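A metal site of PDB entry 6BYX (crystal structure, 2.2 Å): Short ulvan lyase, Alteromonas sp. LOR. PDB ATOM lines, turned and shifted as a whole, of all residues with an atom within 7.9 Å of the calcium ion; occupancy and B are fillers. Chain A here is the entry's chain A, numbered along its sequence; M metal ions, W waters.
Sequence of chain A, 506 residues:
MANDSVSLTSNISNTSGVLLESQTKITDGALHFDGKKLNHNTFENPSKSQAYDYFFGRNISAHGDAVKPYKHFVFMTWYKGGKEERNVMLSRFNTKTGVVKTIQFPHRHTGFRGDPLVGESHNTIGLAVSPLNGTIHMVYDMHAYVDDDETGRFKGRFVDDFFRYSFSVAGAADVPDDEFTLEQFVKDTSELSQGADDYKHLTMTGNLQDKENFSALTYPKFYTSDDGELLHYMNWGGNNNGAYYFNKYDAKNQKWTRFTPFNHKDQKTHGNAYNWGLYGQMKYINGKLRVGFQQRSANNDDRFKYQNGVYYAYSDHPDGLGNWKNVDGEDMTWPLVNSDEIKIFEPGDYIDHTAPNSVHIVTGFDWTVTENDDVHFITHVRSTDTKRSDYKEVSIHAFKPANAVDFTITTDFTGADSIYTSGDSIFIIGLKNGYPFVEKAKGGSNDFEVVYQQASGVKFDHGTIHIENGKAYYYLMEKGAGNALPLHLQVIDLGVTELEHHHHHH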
ATOM      1  N   ASN A 240      19.004  36.065  -2.423  1.00  0.00           N
ATOM      2  CA  ASN A 240      17.924  36.249  -1.465  1.00  0.00           C
ATOM      3  C   ASN A 240      17.644  37.725  -1.183  1.00  0.00           C
ATOM      4  O   ASN A 240      17.102  38.064  -0.130  1.00  0.00           O
ATOM      5  CB  ASN A 240      18.214  35.499  -0.177  1.00  0.00           C
ATOM      6  CG  ASN A 240      19.583  35.787   0.350  1.00  0.00           C
ATOM      7  OD1 ASN A 240      20.116  36.878   0.140  1.00  0.00           O
ATOM      8  ND2 ASN A 240      20.171  34.823   1.027  1.00  0.00           N
ATOM      9  N   ARG A 296      13.038  33.666  -2.840  1.00  0.00           N
ATOM     10  CA  ARG A 296      14.137  33.052  -2.085  1.00  0.00           C
ATOM     11  C   ARG A 296      14.355  33.884  -0.817  1.00  0.00           C
ATOM     12  O   ARG A 296      15.036  34.923  -0.830  1.00  0.00           O
ATOM     13  CB  ARG A 296      15.417  32.938  -2.911  1.00  0.00           C
ATOM     14  CG  ARG A 296      16.509  32.206  -2.129  1.00  0.00           C
ATOM     15  CD  ARG A 296      17.808  32.131  -2.873  1.00  0.00           C
ATOM     16  NE  ARG A 296      17.714  31.360  -4.121  1.00  0.00           N
ATOM     17  CZ  ARG A 296      18.769  30.999  -4.840  1.00  0.00           C
ATOM     18  NH1 ARG A 296      19.998  31.328  -4.438  1.00  0.00           N
ATOM     19  NH2 ARG A 296      18.616  30.299  -5.945  1.00  0.00           N
ATOM     20  N   SER A 297      13.806  33.430   0.298  1.00  0.00           N
ATOM     21  CA  SER A 297      14.057  34.114   1.550  1.00  0.00           C
ATOM     22  C   SER A 297      15.533  33.991   1.927  1.00  0.00           C
ATOM     23  O   SER A 297      16.180  32.999   1.621  1.00  0.00           O
ATOM     24  CB  SER A 297      13.201  33.537   2.655  1.00  0.00           C
ATOM     25  OG  SER A 297      13.765  33.871   3.903  1.00  0.00           O
ATOM     26  N   ALA A 298      16.056  35.027   2.590  1.00  0.00           N
ATOM     27  CA  ALA A 298      17.403  34.947   3.170  1.00  0.00           C
ATOM     28  C   ALA A 298      17.464  34.042   4.386  1.00  0.00           C
ATOM     29  O   ALA A 298      18.567  33.766   4.870  1.00  0.00           O
ATOM     30  CB  ALA A 298      17.914  36.331   3.591  1.00  0.00           C
ATOM     31  N   ASN A 299      16.323  33.580   4.898  1.00  0.00           N
ATOM     32  CA  ASN A 299      16.338  32.613   5.996  1.00  0.00           C
ATOM     33  C   ASN A 299      16.931  31.295   5.492  1.00  0.00           C
ATOM     34  O   ASN A 299      16.457  30.741   4.490  1.00  0.00           O
ATOM     35  CB  ASN A 299      14.936  32.413   6.545  1.00  0.00           C
ATOM     36  CG  ASN A 299      14.887  31.397   7.648  1.00  0.00           C
ATOM     37  OD1 ASN A 299      15.927  30.901   8.098  1.00  0.00           O
ATOM     38  ND2 ASN A 299      13.675  31.041   8.069  1.00  0.00           N
ATOM     39  N   ASN A 300      17.976  30.829   6.165  1.00  0.00           N
ATOM     40  CA  ASN A 300      18.695  29.603   5.846  1.00  0.00           C
ATOM     41  C   ASN A 300      18.514  28.523   6.899  1.00  0.00           C
ATOM     42  O   ASN A 300      19.261  27.534   6.910  1.00  0.00           O
ATOM     43  CB  ASN A 300      20.189  29.880   5.648  1.00  0.00           C
ATOM     44  CG  ASN A 300      20.457  30.751   4.423  1.00  0.00           C
ATOM     45  OD1 ASN A 300      19.779  30.638   3.405  1.00  0.00           O
ATOM     46  ND2 ASN A 300      21.427  31.640   4.527  1.00  0.00           N
ATOM     47  N   ASP A 301      17.549  28.695   7.803  1.00  0.00           N
ATOM     48  CA  ASP A 301      17.280  27.700   8.817  1.00  0.00           C
ATOM     49  C   ASP A 301      15.929  27.033   8.649  1.00  0.00           C
ATOM     50  O   ASP A 301      15.624  26.092   9.386  1.00  0.00           O
ATOM     51  CB  ASP A 301      17.373  28.350  10.210  1.00  0.00           C
ATOM     52  CG  ASP A 301      18.757  28.957  10.494  1.00  0.00           C
ATOM     53  OD1 ASP A 301      19.799  28.474   9.961  1.00  0.00           O
ATOM     54  OD2 ASP A 301      18.795  29.928  11.273  1.00  0.00           O
ATOM     55  N   ASP A 302      15.111  27.498   7.707  1.00  0.00           N
ATOM     56  CA  ASP A 302      13.840  26.861   7.402  1.00  0.00           C
ATOM     57  C   ASP A 302      14.076  25.708   6.428  1.00  0.00           C
ATOM     58  O   ASP A 302      15.199  25.431   6.009  1.00  0.00           O
ATOM     59  CB  ASP A 302      12.847  27.888   6.868  1.00  0.00           C
ATOM     60  CG  ASP A 302      13.182  28.367   5.470  1.00  0.00           C
ATOM     61  OD1 ASP A 302      14.135  27.835   4.859  1.00  0.00           O
ATOM     62  OD2 ASP A 302      12.471  29.259   4.967  1.00  0.00           O
ATOM     63  N   ARG A 303      12.987  25.071   6.009  1.00  0.00           N
ATOM     64  CA  ARG A 303      13.069  23.829   5.231  1.00  0.00           C
ATOM     65  C   ARG A 303      13.459  24.035   3.760  1.00  0.00           C
ATOM     66  O   ARG A 303      13.728  23.043   3.073  1.00  0.00           O
ATOM     67  CB  ARG A 303      11.746  23.077   5.297  1.00  0.00           C
ATOM     68  CG  ARG A 303      10.633  23.685   4.410  1.00  0.00           C
ATOM     69  CD  ARG A 303       9.337  22.921   4.622  1.00  0.00           C
ATOM     70  NE  ARG A 303       8.767  23.174   5.938  1.00  0.00           N
ATOM     71  CZ  ARG A 303       7.707  22.557   6.424  1.00  0.00           C
ATOM     72  NH1 ARG A 303       7.059  21.642   5.704  1.00  0.00           N
ATOM     73  NH2 ARG A 303       7.280  22.841   7.655  1.00  0.00           N
ATOM     74  N   PHE A 304      13.472  25.263   3.257  1.00  0.00           N
ATOM     75  CA  PHE A 304      13.664  25.514   1.821  1.00  0.00           C
ATOM     76  C   PHE A 304      15.106  25.941   1.528  1.00  0.00           C
ATOM     77  O   PHE A 304      15.519  27.028   1.940  1.00  0.00           O
ATOM     78  CB  PHE A 304      12.689  26.569   1.337  1.00  0.00           C
ATOM     79  CG  PHE A 304      11.264  26.230   1.598  1.00  0.00           C
ATOM     80  CD1 PHE A 304      10.577  25.340   0.768  1.00  0.00           C
ATOM     81  CD2 PHE A 304      10.599  26.780   2.675  1.00  0.00           C
ATOM     82  CE1 PHE A 304       9.262  25.021   1.024  1.00  0.00           C
ATOM     83  CE2 PHE A 304       9.281  26.473   2.940  1.00  0.00           C
ATOM     84  CZ  PHE A 304       8.593  25.596   2.105  1.00  0.00           C
ATOM     85  N   LYS A 305      15.854  25.099   0.813  1.00  0.00           N
ATOM     86  CA  LYS A 305      17.232  25.467   0.494  1.00  0.00           C
ATOM     87  C   LYS A 305      17.280  26.725  -0.361  1.00  0.00           C
ATOM     88  O   LYS A 305      18.099  27.614  -0.109  1.00  0.00           O
ATOM     89  CB  LYS A 305      17.938  24.324  -0.210  1.00  0.00           C
ATOM     90  CG  LYS A 305      19.372  24.640  -0.597  1.00  0.00           C
ATOM     91  CD  LYS A 305      20.324  24.195   0.497  1.00  0.00           C
ATOM     92  CE  LYS A 305      21.808  24.429   0.166  1.00  0.00           C
ATOM     93  NZ  LYS A 305      22.415  25.593   0.914  1.00  0.00           N
ATOM     94  N   TYR A 306      16.394  26.825  -1.336  1.00  0.00           N
ATOM     95  CA  TYR A 306      16.362  27.984  -2.241  1.00  0.00           C
ATOM     96  C   TYR A 306      14.974  28.590  -2.250  1.00  0.00           C
ATOM     97  O   TYR A 306      14.559  29.232  -1.277  1.00  0.00           O
ATOM     98  CB  TYR A 306      16.818  27.575  -3.651  1.00  0.00           C
ATOM     99  CG  TYR A 306      18.282  27.150  -3.657  1.00  0.00           C
ATOM    100  CD1 TYR A 306      19.262  28.012  -3.202  1.00  0.00           C
ATOM    101  CD2 TYR A 306      18.664  25.876  -4.085  1.00  0.00           C
ATOM    102  CE1 TYR A 306      20.596  27.642  -3.178  1.00  0.00           C
ATOM    103  CE2 TYR A 306      20.024  25.491  -4.067  1.00  0.00           C
ATOM    104  CZ  TYR A 306      20.977  26.395  -3.615  1.00  0.00           C
ATOM    105  OH  TYR A 306      22.311  26.077  -3.552  1.00  0.00           O
ATOM    106  N   GLN A 307      14.218  28.367  -3.327  1.00  0.00           N
ATOM    107  CA  GLN A 307      12.950  29.065  -3.435  1.00  0.00           C
ATOM    108  C   GLN A 307      11.877  28.385  -2.607  1.00  0.00           C
ATOM    109  O   GLN A 307      12.042  27.245  -2.146  1.00  0.00           O
ATOM    110  CB  GLN A 307      12.501  29.157  -4.901  1.00  0.00           C
ATOM    111  CG  GLN A 307      13.195  30.261  -5.697  1.00  0.00           C
ATOM    112  CD  GLN A 307      14.530  29.823  -6.264  1.00  0.00           C
ATOM    113  OE1 GLN A 307      15.570  29.972  -5.622  1.00  0.00           O
ATOM    114  NE2 GLN A 307      14.502  29.289  -7.475  1.00  0.00           N
ATOM    115  N   ASN A 308      10.785  29.115  -2.375  1.00  0.00           N
ATOM    116  CA  ASN A 308       9.554  28.542  -1.845  1.00  0.00           C
ATOM    117  C   ASN A 308       8.386  29.374  -2.342  1.00  0.00           C
ATOM    118  O   ASN A 308       8.546  30.493  -2.840  1.00  0.00           O
ATOM    119  CB  ASN A 308       9.531  28.469  -0.303  1.00  0.00           C
ATOM    120  CG  ASN A 308       9.224  29.811   0.356  1.00  0.00           C
ATOM    121  OD1 ASN A 308      10.124  30.626   0.597  1.00  0.00           O
ATOM    122  ND2 ASN A 308       7.952  30.037   0.668  1.00  0.00           N
ATOM    123  N   PRO A 356      15.638  21.493   8.167  1.00  0.00           N
ATOM    124  CA  PRO A 356      16.147  22.690   7.474  1.00  0.00           C
ATOM    125  C   PRO A 356      16.860  22.325   6.154  1.00  0.00           C
ATOM    126  O   PRO A 356      17.644  21.377   6.083  1.00  0.00           O
ATOM    127  CB  PRO A 356      17.103  23.313   8.490  1.00  0.00           C
ATOM    128  CG  PRO A 356      16.662  22.750   9.845  1.00  0.00           C
ATOM    129  CD  PRO A 356      16.184  21.348   9.533  1.00  0.00           C
ATOM    130  N   ASN A 357      16.540  23.086   5.103  1.00  0.00           N
ATOM    131  CA  ASN A 357      17.139  22.997   3.778  1.00  0.00           C
ATOM    132  C   ASN A 357      16.862  21.687   3.066  1.00  0.00           C
ATOM    133  O   ASN A 357      17.519  21.371   2.053  1.00  0.00           O
ATOM    134  CB  ASN A 357      18.655  23.248   3.853  1.00  0.00           C
ATOM    135  CG  ASN A 357      18.957  24.637   4.365  1.00  0.00           C
ATOM    136  OD1 ASN A 357      18.723  25.618   3.670  1.00  0.00           O
ATOM    137  ND2 ASN A 357      19.476  24.736   5.599  1.00  0.00           N
ATOM    138  N   VAL A 359      14.140  20.814   1.386  1.00  0.00           N
ATOM    139  CA  VAL A 359      13.219  20.947   0.260  1.00  0.00           C
ATOM    140  C   VAL A 359      13.838  21.861  -0.791  1.00  0.00           C
ATOM    141  O   VAL A 359      14.159  23.021  -0.492  1.00  0.00           O
ATOM    142  CB  VAL A 359      11.840  21.463   0.699  1.00  0.00           C
ATOM    143  CG1 VAL A 359      10.963  21.725  -0.513  1.00  0.00           C
ATOM    144  CG2 VAL A 359      11.175  20.470   1.650  1.00  0.00           C
HETATM  145 CA    CA M   1      15.775  28.853   3.252  1.00  0.00          CA
HETATM  146  O   HOH W   1      18.203  28.658   2.690  1.00  0.00           O
HETATM  147  O   HOH W   2      16.119  30.095   1.076  1.00  0.00           O
HETATM  148  O   HOH W   3      13.684  29.949   2.898  1.00  0.00           O
HETATM  149  O   HOH W   4      16.917  27.565   4.828  1.00  0.00           O
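OD1 of Asn 299 sits at hydrogen-bond distance from N of Asp 301 (2.8 Å). N of Asn 357 sits at hydrogen-bond distance from O of Asp 302, at 2.8 Å. ND2 of Asn 357 lies within hydrogen-bond range of O of Asn 300 (3.1 Å). N of Asn 299 is in hydrogen-bond range of OG of Ser 297 (2.8 Å).
Asn 300 touches the calcium ion.
O of Phe 304 binds the calcium ion (2.3 Å). The calcium ion is bound by water W4, 2.3 Å away. O of Asn 299 binds the calcium ion (2.4 Å). The calcium ion is bound by water W3, at 2.4 Å. Water W1 is bound to the calcium ion (2.5 Å). The calcium ion is bound by OD1 of Asp 302, at 2.5 Å. The calcium ion is bound by water W2 (2.5 Å).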
